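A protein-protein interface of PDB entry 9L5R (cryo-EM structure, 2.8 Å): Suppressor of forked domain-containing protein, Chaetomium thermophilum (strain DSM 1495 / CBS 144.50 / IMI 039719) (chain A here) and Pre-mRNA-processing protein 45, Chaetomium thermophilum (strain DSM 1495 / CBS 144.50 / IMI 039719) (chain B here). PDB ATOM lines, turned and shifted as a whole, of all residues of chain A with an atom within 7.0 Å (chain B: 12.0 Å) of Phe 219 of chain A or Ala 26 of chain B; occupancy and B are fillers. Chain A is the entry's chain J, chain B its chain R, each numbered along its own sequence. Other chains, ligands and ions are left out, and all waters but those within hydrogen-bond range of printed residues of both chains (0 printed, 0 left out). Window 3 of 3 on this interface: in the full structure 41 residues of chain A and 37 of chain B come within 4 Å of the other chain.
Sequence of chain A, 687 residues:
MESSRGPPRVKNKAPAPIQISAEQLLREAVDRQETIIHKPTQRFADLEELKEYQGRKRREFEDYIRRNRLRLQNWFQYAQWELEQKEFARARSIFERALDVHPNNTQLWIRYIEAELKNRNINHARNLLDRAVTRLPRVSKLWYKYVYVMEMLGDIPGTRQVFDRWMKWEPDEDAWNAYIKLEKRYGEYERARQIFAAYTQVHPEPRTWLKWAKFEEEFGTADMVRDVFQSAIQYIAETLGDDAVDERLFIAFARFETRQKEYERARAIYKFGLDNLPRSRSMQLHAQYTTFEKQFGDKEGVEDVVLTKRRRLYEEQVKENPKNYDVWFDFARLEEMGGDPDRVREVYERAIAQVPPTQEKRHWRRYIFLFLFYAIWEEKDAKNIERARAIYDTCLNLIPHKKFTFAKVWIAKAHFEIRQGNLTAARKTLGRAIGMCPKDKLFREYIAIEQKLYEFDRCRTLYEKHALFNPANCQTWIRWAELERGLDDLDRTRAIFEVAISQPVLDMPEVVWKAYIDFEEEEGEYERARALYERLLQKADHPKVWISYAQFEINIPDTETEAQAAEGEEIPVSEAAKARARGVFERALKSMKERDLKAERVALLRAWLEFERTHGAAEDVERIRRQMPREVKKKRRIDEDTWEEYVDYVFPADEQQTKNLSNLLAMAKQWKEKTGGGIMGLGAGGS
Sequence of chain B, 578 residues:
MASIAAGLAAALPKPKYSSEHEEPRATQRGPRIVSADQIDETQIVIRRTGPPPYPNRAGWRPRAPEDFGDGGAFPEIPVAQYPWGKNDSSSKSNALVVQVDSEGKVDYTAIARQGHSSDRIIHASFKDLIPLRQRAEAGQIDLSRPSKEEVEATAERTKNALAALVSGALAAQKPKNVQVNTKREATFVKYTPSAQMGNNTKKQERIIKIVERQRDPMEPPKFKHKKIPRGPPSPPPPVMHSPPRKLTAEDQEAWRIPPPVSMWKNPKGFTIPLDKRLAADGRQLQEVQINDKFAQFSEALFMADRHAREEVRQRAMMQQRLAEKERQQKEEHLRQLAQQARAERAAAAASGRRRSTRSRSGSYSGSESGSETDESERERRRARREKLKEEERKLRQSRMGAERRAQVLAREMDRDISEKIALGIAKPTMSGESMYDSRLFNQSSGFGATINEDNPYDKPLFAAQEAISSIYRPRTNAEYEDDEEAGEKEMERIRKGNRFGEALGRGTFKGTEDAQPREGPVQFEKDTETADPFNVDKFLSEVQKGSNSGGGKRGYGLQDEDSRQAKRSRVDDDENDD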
ATOM      1  N   LYS A 184      -1.928   5.075  13.685  1.00  0.00           N
ATOM      2  CA  LYS A 184      -2.722   6.238  14.065  1.00  0.00           C
ATOM      3  C   LYS A 184      -3.746   6.602  13.003  1.00  0.00           C
ATOM      4  O   LYS A 184      -4.830   7.081  13.341  1.00  0.00           O
ATOM      5  CB  LYS A 184      -1.819   7.431  14.343  1.00  0.00           C
ATOM      6  CG  LYS A 184      -0.963   7.268  15.554  1.00  0.00           C
ATOM      7  CD  LYS A 184      -0.578   8.598  16.116  1.00  0.00           C
ATOM      8  CE  LYS A 184       0.201   9.410  15.121  1.00  0.00           C
ATOM      9  NZ  LYS A 184       0.641  10.697  15.708  1.00  0.00           N
ATOM     10  N   TYR A 189      -4.363   3.006  18.582  1.00  0.00           N
ATOM     11  CA  TYR A 189      -3.411   3.726  19.408  1.00  0.00           C
ATOM     12  C   TYR A 189      -2.635   2.797  20.321  1.00  0.00           C
ATOM     13  O   TYR A 189      -1.479   3.081  20.643  1.00  0.00           O
ATOM     14  CB  TYR A 189      -4.149   4.794  20.194  1.00  0.00           C
ATOM     15  CG  TYR A 189      -4.956   5.669  19.283  1.00  0.00           C
ATOM     16  CD1 TYR A 189      -4.351   6.342  18.239  1.00  0.00           C
ATOM     17  CD2 TYR A 189      -6.320   5.808  19.448  1.00  0.00           C
ATOM     18  CE1 TYR A 189      -5.073   7.132  17.395  1.00  0.00           C
ATOM     19  CE2 TYR A 189      -7.052   6.603  18.604  1.00  0.00           C
ATOM     20  CZ  TYR A 189      -6.422   7.261  17.580  1.00  0.00           C
ATOM     21  OH  TYR A 189      -7.146   8.055  16.732  1.00  0.00           O
ATOM     22  N   ARG A 193       1.336   2.409  20.438  1.00  0.00           N
ATOM     23  CA  ARG A 193       2.061   2.343  21.705  1.00  0.00           C
ATOM     24  C   ARG A 193       3.076   1.206  21.709  1.00  0.00           C
ATOM     25  O   ARG A 193       4.215   1.367  22.174  1.00  0.00           O
ATOM     26  CB  ARG A 193       1.049   2.166  22.833  1.00  0.00           C
ATOM     27  CG  ARG A 193       1.483   2.594  24.196  1.00  0.00           C
ATOM     28  CD  ARG A 193       0.287   2.658  25.115  1.00  0.00           C
ATOM     29  NE  ARG A 193      -0.538   3.821  24.821  1.00  0.00           N
ATOM     30  CZ  ARG A 193      -1.842   3.778  24.607  1.00  0.00           C
ATOM     31  NH1 ARG A 193      -2.517   2.649  24.689  1.00  0.00           N
ATOM     32  NH2 ARG A 193      -2.482   4.894  24.292  1.00  0.00           N
ATOM     33  N   LYS A 214       4.980  12.873  23.492  1.00  0.00           N
ATOM     34  CA  LYS A 214       3.968  13.673  22.808  1.00  0.00           C
ATOM     35  C   LYS A 214       2.790  12.814  22.361  1.00  0.00           C
ATOM     36  O   LYS A 214       1.626  13.237  22.459  1.00  0.00           O
ATOM     37  CB  LYS A 214       4.605  14.391  21.625  1.00  0.00           C
ATOM     38  CG  LYS A 214       3.628  15.086  20.723  1.00  0.00           C
ATOM     39  CD  LYS A 214       4.324  15.763  19.564  1.00  0.00           C
ATOM     40  CE  LYS A 214       4.893  17.108  19.966  1.00  0.00           C
ATOM     41  NZ  LYS A 214       4.864  18.069  18.836  1.00  0.00           N
ATOM     42  N   PHE A 215       3.074  11.591  21.898  1.00  0.00           N
ATOM     43  CA  PHE A 215       2.014  10.649  21.560  1.00  0.00           C
ATOM     44  C   PHE A 215       1.119  10.371  22.749  1.00  0.00           C
ATOM     45  O   PHE A 215      -0.104  10.339  22.616  1.00  0.00           O
ATOM     46  CB  PHE A 215       2.612   9.340  21.057  1.00  0.00           C
ATOM     47  CG  PHE A 215       1.606   8.245  20.872  1.00  0.00           C
ATOM     48  CD1 PHE A 215       0.834   8.197  19.738  1.00  0.00           C
ATOM     49  CD2 PHE A 215       1.452   7.252  21.818  1.00  0.00           C
ATOM     50  CE1 PHE A 215      -0.080   7.205  19.564  1.00  0.00           C
ATOM     51  CE2 PHE A 215       0.535   6.267  21.649  1.00  0.00           C
ATOM     52  CZ  PHE A 215      -0.229   6.241  20.518  1.00  0.00           C
ATOM     53  N   GLU A 216       1.710  10.133  23.914  1.00  0.00           N
ATOM     54  CA  GLU A 216       0.895   9.793  25.068  1.00  0.00           C
ATOM     55  C   GLU A 216       0.167  11.003  25.613  1.00  0.00           C
ATOM     56  O   GLU A 216      -0.896  10.860  26.219  1.00  0.00           O
ATOM     57  CB  GLU A 216       1.745   9.156  26.157  1.00  0.00           C
ATOM     58  CG  GLU A 216       2.427   7.897  25.734  1.00  0.00           C
ATOM     59  CD  GLU A 216       1.571   6.662  25.885  1.00  0.00           C
ATOM     60  OE1 GLU A 216       0.373   6.689  25.546  1.00  0.00           O
ATOM     61  OE2 GLU A 216       2.108   5.638  26.343  1.00  0.00           O
ATOM     62  N   GLU A 217       0.723  12.196  25.427  1.00  0.00           N
ATOM     63  CA  GLU A 217      -0.013  13.398  25.787  1.00  0.00           C
ATOM     64  C   GLU A 217      -1.242  13.576  24.916  1.00  0.00           C
ATOM     65  O   GLU A 217      -2.249  14.122  25.371  1.00  0.00           O
ATOM     66  CB  GLU A 217       0.894  14.614  25.681  1.00  0.00           C
ATOM     67  CG  GLU A 217       0.322  15.859  26.296  1.00  0.00           C
ATOM     68  CD  GLU A 217       1.367  16.918  26.492  1.00  0.00           C
ATOM     69  OE1 GLU A 217       2.524  16.683  26.091  1.00  0.00           O
ATOM     70  OE2 GLU A 217       1.040  17.983  27.048  1.00  0.00           O
ATOM     71  N   GLU A 218      -1.187  13.134  23.664  1.00  0.00           N
ATOM     72  CA  GLU A 218      -2.381  13.265  22.839  1.00  0.00           C
ATOM     73  C   GLU A 218      -3.357  12.107  23.019  1.00  0.00           C
ATOM     74  O   GLU A 218      -4.571  12.321  23.048  1.00  0.00           O
ATOM     75  CB  GLU A 218      -1.993  13.393  21.375  1.00  0.00           C
ATOM     76  CG  GLU A 218      -3.142  13.806  20.489  1.00  0.00           C
ATOM     77  CD  GLU A 218      -2.702  14.081  19.080  1.00  0.00           C
ATOM     78  OE1 GLU A 218      -1.497  14.336  18.877  1.00  0.00           O
ATOM     79  OE2 GLU A 218      -3.558  14.050  18.177  1.00  0.00           O
ATOM     80  N   PHE A 219      -2.861  10.877  23.138  1.00  0.00           N
ATOM     81  CA  PHE A 219      -3.697   9.686  23.028  1.00  0.00           C
ATOM     82  C   PHE A 219      -3.708   8.821  24.275  1.00  0.00           C
ATOM     83  O   PHE A 219      -4.228   7.706  24.226  1.00  0.00           O
ATOM     84  CB  PHE A 219      -3.249   8.826  21.846  1.00  0.00           C
ATOM     85  CG  PHE A 219      -3.371   9.504  20.530  1.00  0.00           C
ATOM     86  CD1 PHE A 219      -4.601   9.682  19.952  1.00  0.00           C
ATOM     87  CD2 PHE A 219      -2.255   9.965  19.870  1.00  0.00           C
ATOM     88  CE1 PHE A 219      -4.722  10.312  18.756  1.00  0.00           C
ATOM     89  CE2 PHE A 219      -2.370  10.590  18.665  1.00  0.00           C
ATOM     90  CZ  PHE A 219      -3.605  10.760  18.105  1.00  0.00           C
ATOM     91  N   GLY A 220      -3.155   9.284  25.374  1.00  0.00           N
ATOM     92  CA  GLY A 220      -3.042   8.449  26.553  1.00  0.00           C
ATOM     93  C   GLY A 220      -3.551   9.158  27.786  1.00  0.00           C
ATOM     94  O   GLY A 220      -4.539   9.873  27.755  1.00  0.00           O
ATOM     95  N   THR A 221      -2.872   8.915  28.899  1.00  0.00           N
ATOM     96  CA  THR A 221      -3.158   9.571  30.161  1.00  0.00           C
ATOM     97  C   THR A 221      -1.893  10.244  30.670  1.00  0.00           C
ATOM     98  O   THR A 221      -0.780   9.904  30.261  1.00  0.00           O
ATOM     99  CB  THR A 221      -3.684   8.584  31.214  1.00  0.00           C
ATOM    100  OG1 THR A 221      -2.614   7.760  31.682  1.00  0.00           O
ATOM    101  CG2 THR A 221      -4.782   7.709  30.644  1.00  0.00           C
ATOM    102  N   MET A 224       0.654   7.933  32.001  1.00  0.00           N
ATOM    103  CA  MET A 224       1.531   7.298  31.025  1.00  0.00           C
ATOM    104  C   MET A 224       2.519   8.274  30.408  1.00  0.00           C
ATOM    105  O   MET A 224       3.626   7.862  30.059  1.00  0.00           O
ATOM    106  CB  MET A 224       0.736   6.559  29.949  1.00  0.00           C
ATOM    107  CG  MET A 224      -0.058   5.402  30.525  1.00  0.00           C
ATOM    108  SD  MET A 224      -1.024   4.424  29.370  1.00  0.00           S
ATOM    109  CE  MET A 224      -1.785   5.689  28.409  1.00  0.00           C
ATOM    110  N   HIS B  21      -8.869   8.574  37.856  1.00  0.00           N
ATOM    111  CA  HIS B  21     -10.137   8.404  37.162  1.00  0.00           C
ATOM    112  C   HIS B  21     -10.050   8.790  35.693  1.00  0.00           C
ATOM    113  O   HIS B  21     -11.084   8.961  35.042  1.00  0.00           O
ATOM    114  CB  HIS B  21     -11.230   9.218  37.852  1.00  0.00           C
ATOM    115  CG  HIS B  21     -11.981   8.457  38.901  1.00  0.00           C
ATOM    116  ND1 HIS B  21     -11.601   8.443  40.225  1.00  0.00           N
ATOM    117  CD2 HIS B  21     -13.094   7.691  38.820  1.00  0.00           C
ATOM    118  CE1 HIS B  21     -12.445   7.697  40.915  1.00  0.00           C
ATOM    119  NE2 HIS B  21     -13.361   7.230  40.087  1.00  0.00           N
ATOM    120  N   GLU B  22      -8.841   8.924  35.156  1.00  0.00           N
ATOM    121  CA  GLU B  22      -8.647   9.445  33.809  1.00  0.00           C
ATOM    122  C   GLU B  22      -8.756   8.321  32.789  1.00  0.00           C
ATOM    123  O   GLU B  22      -8.031   7.324  32.871  1.00  0.00           O
ATOM    124  CB  GLU B  22      -7.294  10.144  33.687  1.00  0.00           C
ATOM    125  CG  GLU B  22      -7.148  10.975  32.423  1.00  0.00           C
ATOM    126  CD  GLU B  22      -5.844  11.739  32.369  1.00  0.00           C
ATOM    127  OE1 GLU B  22      -5.007  11.549  33.273  1.00  0.00           O
ATOM    128  OE2 GLU B  22      -5.657  12.528  31.421  1.00  0.00           O
ATOM    129  N   GLU B  23      -9.669   8.483  31.842  1.00  0.00           N
ATOM    130  CA  GLU B  23      -9.736   7.655  30.650  1.00  0.00           C
ATOM    131  C   GLU B  23      -8.717   8.169  29.641  1.00  0.00           C
ATOM    132  O   GLU B  23      -8.185   9.269  29.804  1.00  0.00           O
ATOM    133  CB  GLU B  23     -11.158   7.682  30.093  1.00  0.00           C
ATOM    134  CG  GLU B  23     -12.208   7.108  31.035  1.00  0.00           C
ATOM    135  CD  GLU B  23     -12.788   8.148  31.979  1.00  0.00           C
ATOM    136  OE1 GLU B  23     -13.016   9.293  31.535  1.00  0.00           O
ATOM    137  OE2 GLU B  23     -13.011   7.822  33.164  1.00  0.00           O
ATOM    138  N   PRO B  24      -8.375   7.375  28.621  1.00  0.00           N
ATOM    139  CA  PRO B  24      -7.467   7.874  27.576  1.00  0.00           C
ATOM    140  C   PRO B  24      -8.021   9.098  26.862  1.00  0.00           C
ATOM    141  O   PRO B  24      -9.230   9.235  26.661  1.00  0.00           O
ATOM    142  CB  PRO B  24      -7.332   6.685  26.622  1.00  0.00           C
ATOM    143  CG  PRO B  24      -7.680   5.505  27.405  1.00  0.00           C
ATOM    144  CD  PRO B  24      -8.473   5.906  28.606  1.00  0.00           C
ATOM    145  N   ARG B  25      -7.115   9.993  26.481  1.00  0.00           N
ATOM    146  CA  ARG B  25      -7.476  11.284  25.910  1.00  0.00           C
ATOM    147  C   ARG B  25      -8.033  11.181  24.498  1.00  0.00           C
ATOM    148  O   ARG B  25      -8.513  12.187  23.966  1.00  0.00           O
ATOM    149  CB  ARG B  25      -6.263  12.214  25.940  1.00  0.00           C
ATOM    150  CG  ARG B  25      -5.933  12.678  27.339  1.00  0.00           C
ATOM    151  CD  ARG B  25      -4.565  13.300  27.439  1.00  0.00           C
ATOM    152  NE  ARG B  25      -4.307  13.771  28.794  1.00  0.00           N
ATOM    153  CZ  ARG B  25      -3.328  14.597  29.136  1.00  0.00           C
ATOM    154  NH1 ARG B  25      -2.502  15.098  28.238  1.00  0.00           N
ATOM    155  NH2 ARG B  25      -3.185  14.936  30.411  1.00  0.00           N
ATOM    156  N   ALA B  26      -7.979  10.007  23.880  1.00  0.00           N
ATOM    157  CA  ALA B  26      -8.684   9.764  22.630  1.00  0.00           C
ATOM    158  C   ALA B  26      -9.145   8.319  22.634  1.00  0.00           C
ATOM    159  O   ALA B  26      -8.323   7.407  22.747  1.00  0.00           O
ATOM    160  CB  ALA B  26      -7.802  10.052  21.422  1.00  0.00           C
ATOM    161  N   THR B  27     -10.453   8.125  22.512  1.00  0.00           N
ATOM    162  CA  THR B  27     -11.042   6.806  22.679  1.00  0.00           C
ATOM    163  C   THR B  27     -10.812   5.937  21.450  1.00  0.00           C
ATOM    164  O   THR B  27     -10.730   6.430  20.323  1.00  0.00           O
ATOM    165  CB  THR B  27     -12.537   6.930  22.958  1.00  0.00           C
ATOM    166  OG1 THR B  27     -13.136   7.781  21.973  1.00  0.00           O
ATOM    167  CG2 THR B  27     -12.772   7.519  24.338  1.00  0.00           C
ATOM    168  N   GLN B  28     -10.710   4.635  21.684  1.00  0.00           N
ATOM    169  CA  GLN B  28     -10.527   3.643  20.634  1.00  0.00           C
ATOM    170  C   GLN B  28     -11.893   3.126  20.199  1.00  0.00           C
ATOM    171  O   GLN B  28     -12.708   2.741  21.041  1.00  0.00           O
ATOM    172  CB  GLN B  28      -9.649   2.506  21.152  1.00  0.00           C
ATOM    173  CG  GLN B  28      -9.638   1.242  20.315  1.00  0.00           C
ATOM    174  CD  GLN B  28      -8.492   1.205  19.333  1.00  0.00           C
ATOM    175  OE1 GLN B  28      -7.336   1.400  19.705  1.00  0.00           O
ATOM    176  NE2 GLN B  28      -8.804   0.924  18.074  1.00  0.00           N
ATOM    177  N   ARG B  29     -12.143   3.120  18.894  1.00  0.00           N
ATOM    178  CA  ARG B  29     -13.416   2.645  18.361  1.00  0.00           C
ATOM    179  C   ARG B  29     -13.465   1.129  18.491  1.00  0.00           C
ATOM    180  O   ARG B  29     -12.980   0.402  17.625  1.00  0.00           O
ATOM    181  CB  ARG B  29     -13.580   3.084  16.912  1.00  0.00           C
ATOM    182  CG  ARG B  29     -13.770   4.585  16.741  1.00  0.00           C
ATOM    183  CD  ARG B  29     -15.183   4.945  16.288  1.00  0.00           C
ATOM    184  NE  ARG B  29     -15.443   4.591  14.897  1.00  0.00           N
ATOM    185  CZ  ARG B  29     -15.075   5.321  13.853  1.00  0.00           C
ATOM    186  NH1 ARG B  29     -14.426   6.464  14.002  1.00  0.00           N
ATOM    187  NH2 ARG B  29     -15.370   4.898  12.628  1.00  0.00           N
ATOM    188  N   GLY B  30     -14.060   0.645  19.581  1.00  0.00           N
ATOM    189  CA  GLY B  30     -14.081  -0.766  19.895  1.00  0.00           C
ATOM    190  C   GLY B  30     -14.960  -1.558  18.950  1.00  0.00           C
ATOM    191  O   GLY B  30     -15.677  -0.979  18.135  1.00  0.00           O
ATOM    192  N   ARG B  32     -12.688  -4.140  21.636  1.00  0.00           N
ATOM    193  CA  ARG B  32     -11.291  -4.372  21.947  1.00  0.00           C
ATOM    194  C   ARG B  32     -10.893  -5.774  21.524  1.00  0.00           C
ATOM    195  O   ARG B  32     -11.572  -6.749  21.853  1.00  0.00           O
ATOM    196  CB  ARG B  32     -11.041  -4.190  23.438  1.00  0.00           C
ATOM    197  CG  ARG B  32     -11.132  -2.760  23.910  1.00  0.00           C
ATOM    198  CD  ARG B  32     -10.385  -2.592  25.215  1.00  0.00           C
ATOM    199  NE  ARG B  32     -10.491  -3.780  26.050  1.00  0.00           N
ATOM    200  CZ  ARG B  32      -9.461  -4.393  26.613  1.00  0.00           C
ATOM    201  NH1 ARG B  32      -8.222  -3.968  26.431  1.00  0.00           N
ATOM    202  NH2 ARG B  32      -9.677  -5.459  27.376  1.00  0.00           N
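The backbone NH of Arg 25 of chain B sits at hydrogen-bond distance from the backbone carbonyl oxygen of Gly 220 of chain A, 2.9 Å away. The backbone carbonyl oxygen (O) of Glu 217 of chain A sits at hydrogen-bond distance from the guanidinium group (NH1) of Arg 25 of chain B.
The guanidinium group (NH2) of Arg 193 of chain A is in hydrogen-bond range of the backbone carbonyl oxygen (O) of Phe 219 of chain A. OE2 of Glu 22 of chain B is in salt-bridge range of NE of Arg 25 of chain B, at 3.2 Å. The side-chain hydroxyl of Thr 221 of chain A is in hydrogen-bond range of the backbone NH of Met 224 of chain A (3.3 Å).
Tyr 189 of chain A touches Gln 28 of chain B. Glu 218 of chain A touches Arg 25 of chain B (O to CB, 3.4 Å). Phe 219 of chain A touches Ala 26 of chain B (CD1 to CB, 3.5 Å). Gly 220 of chain A touches Pro 24 of chain B. Thr 221 of chain A touches Glu 22 of chain B (CB to OE1, 3.8 Å). Thr 221 of chain A touches Glu 23 of chain B.
Of chain B, only Ala 26 (3.5 Å) comes within 4 Å of Phe 219 of chain A. Ala 26 of chain B touches one residue of chain A. Lys 184 of chain A touches none of the printed residues of chain B. Of chain B, only Gln 28 (3.6 Å) comes within 4 Å of Tyr 189 of chain A. No residue of chain B comes within 4 Å of Phe 215 of chain A. No residue of chain B comes within 4 Å of Glu 216 of chain A. Of chain B, only Arg 25 comes within 4 Å of Glu 218 of chain A. Of the printed residues of chain B, Gly 220 of chain A touches Pro 24 (3.5 Å) and Arg 25 (2.9 Å). Thr 221 of chain A touches just these residues of chain B: Glu 22 (3.8 Å) and Glu 23 (3.8 Å). Printed residues of chain A within 4 Å of Pro 24 of chain B: Gly 220. Printed residues of chain A within 4 Å of Glu 23 of chain B: Thr 221 (3.8 Å). Printed residues of chain B within 4 Å of Glu 217 of chain A: Arg 25 (3.0 Å). Of the printed residues of chain A, Arg 25 of chain B touches Glu 217 (3.0 Å), Glu 218 (3.4 Å) and Gly 220 (2.9 Å). Of the printed residues of chain A, Glu 22 of chain B touches Thr 221. Gly 30 of chain B touches none of the printed residues of chain A.
Hydrophobic or aromatic side chains of chain A that line the printed part of chain B: Phe 219. Printed residues of chain B that touch a printed residue of chain A: Glu 22, Glu 23, Pro 24, Arg 25, Ala 26 and Gln 28. Among the printed residues, 8 pairs touch across the chains. Among the printed residues, no Asp or Glu carboxylate lies within 4 Å of a Lys or Arg side-chain nitrogen of the other chain.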
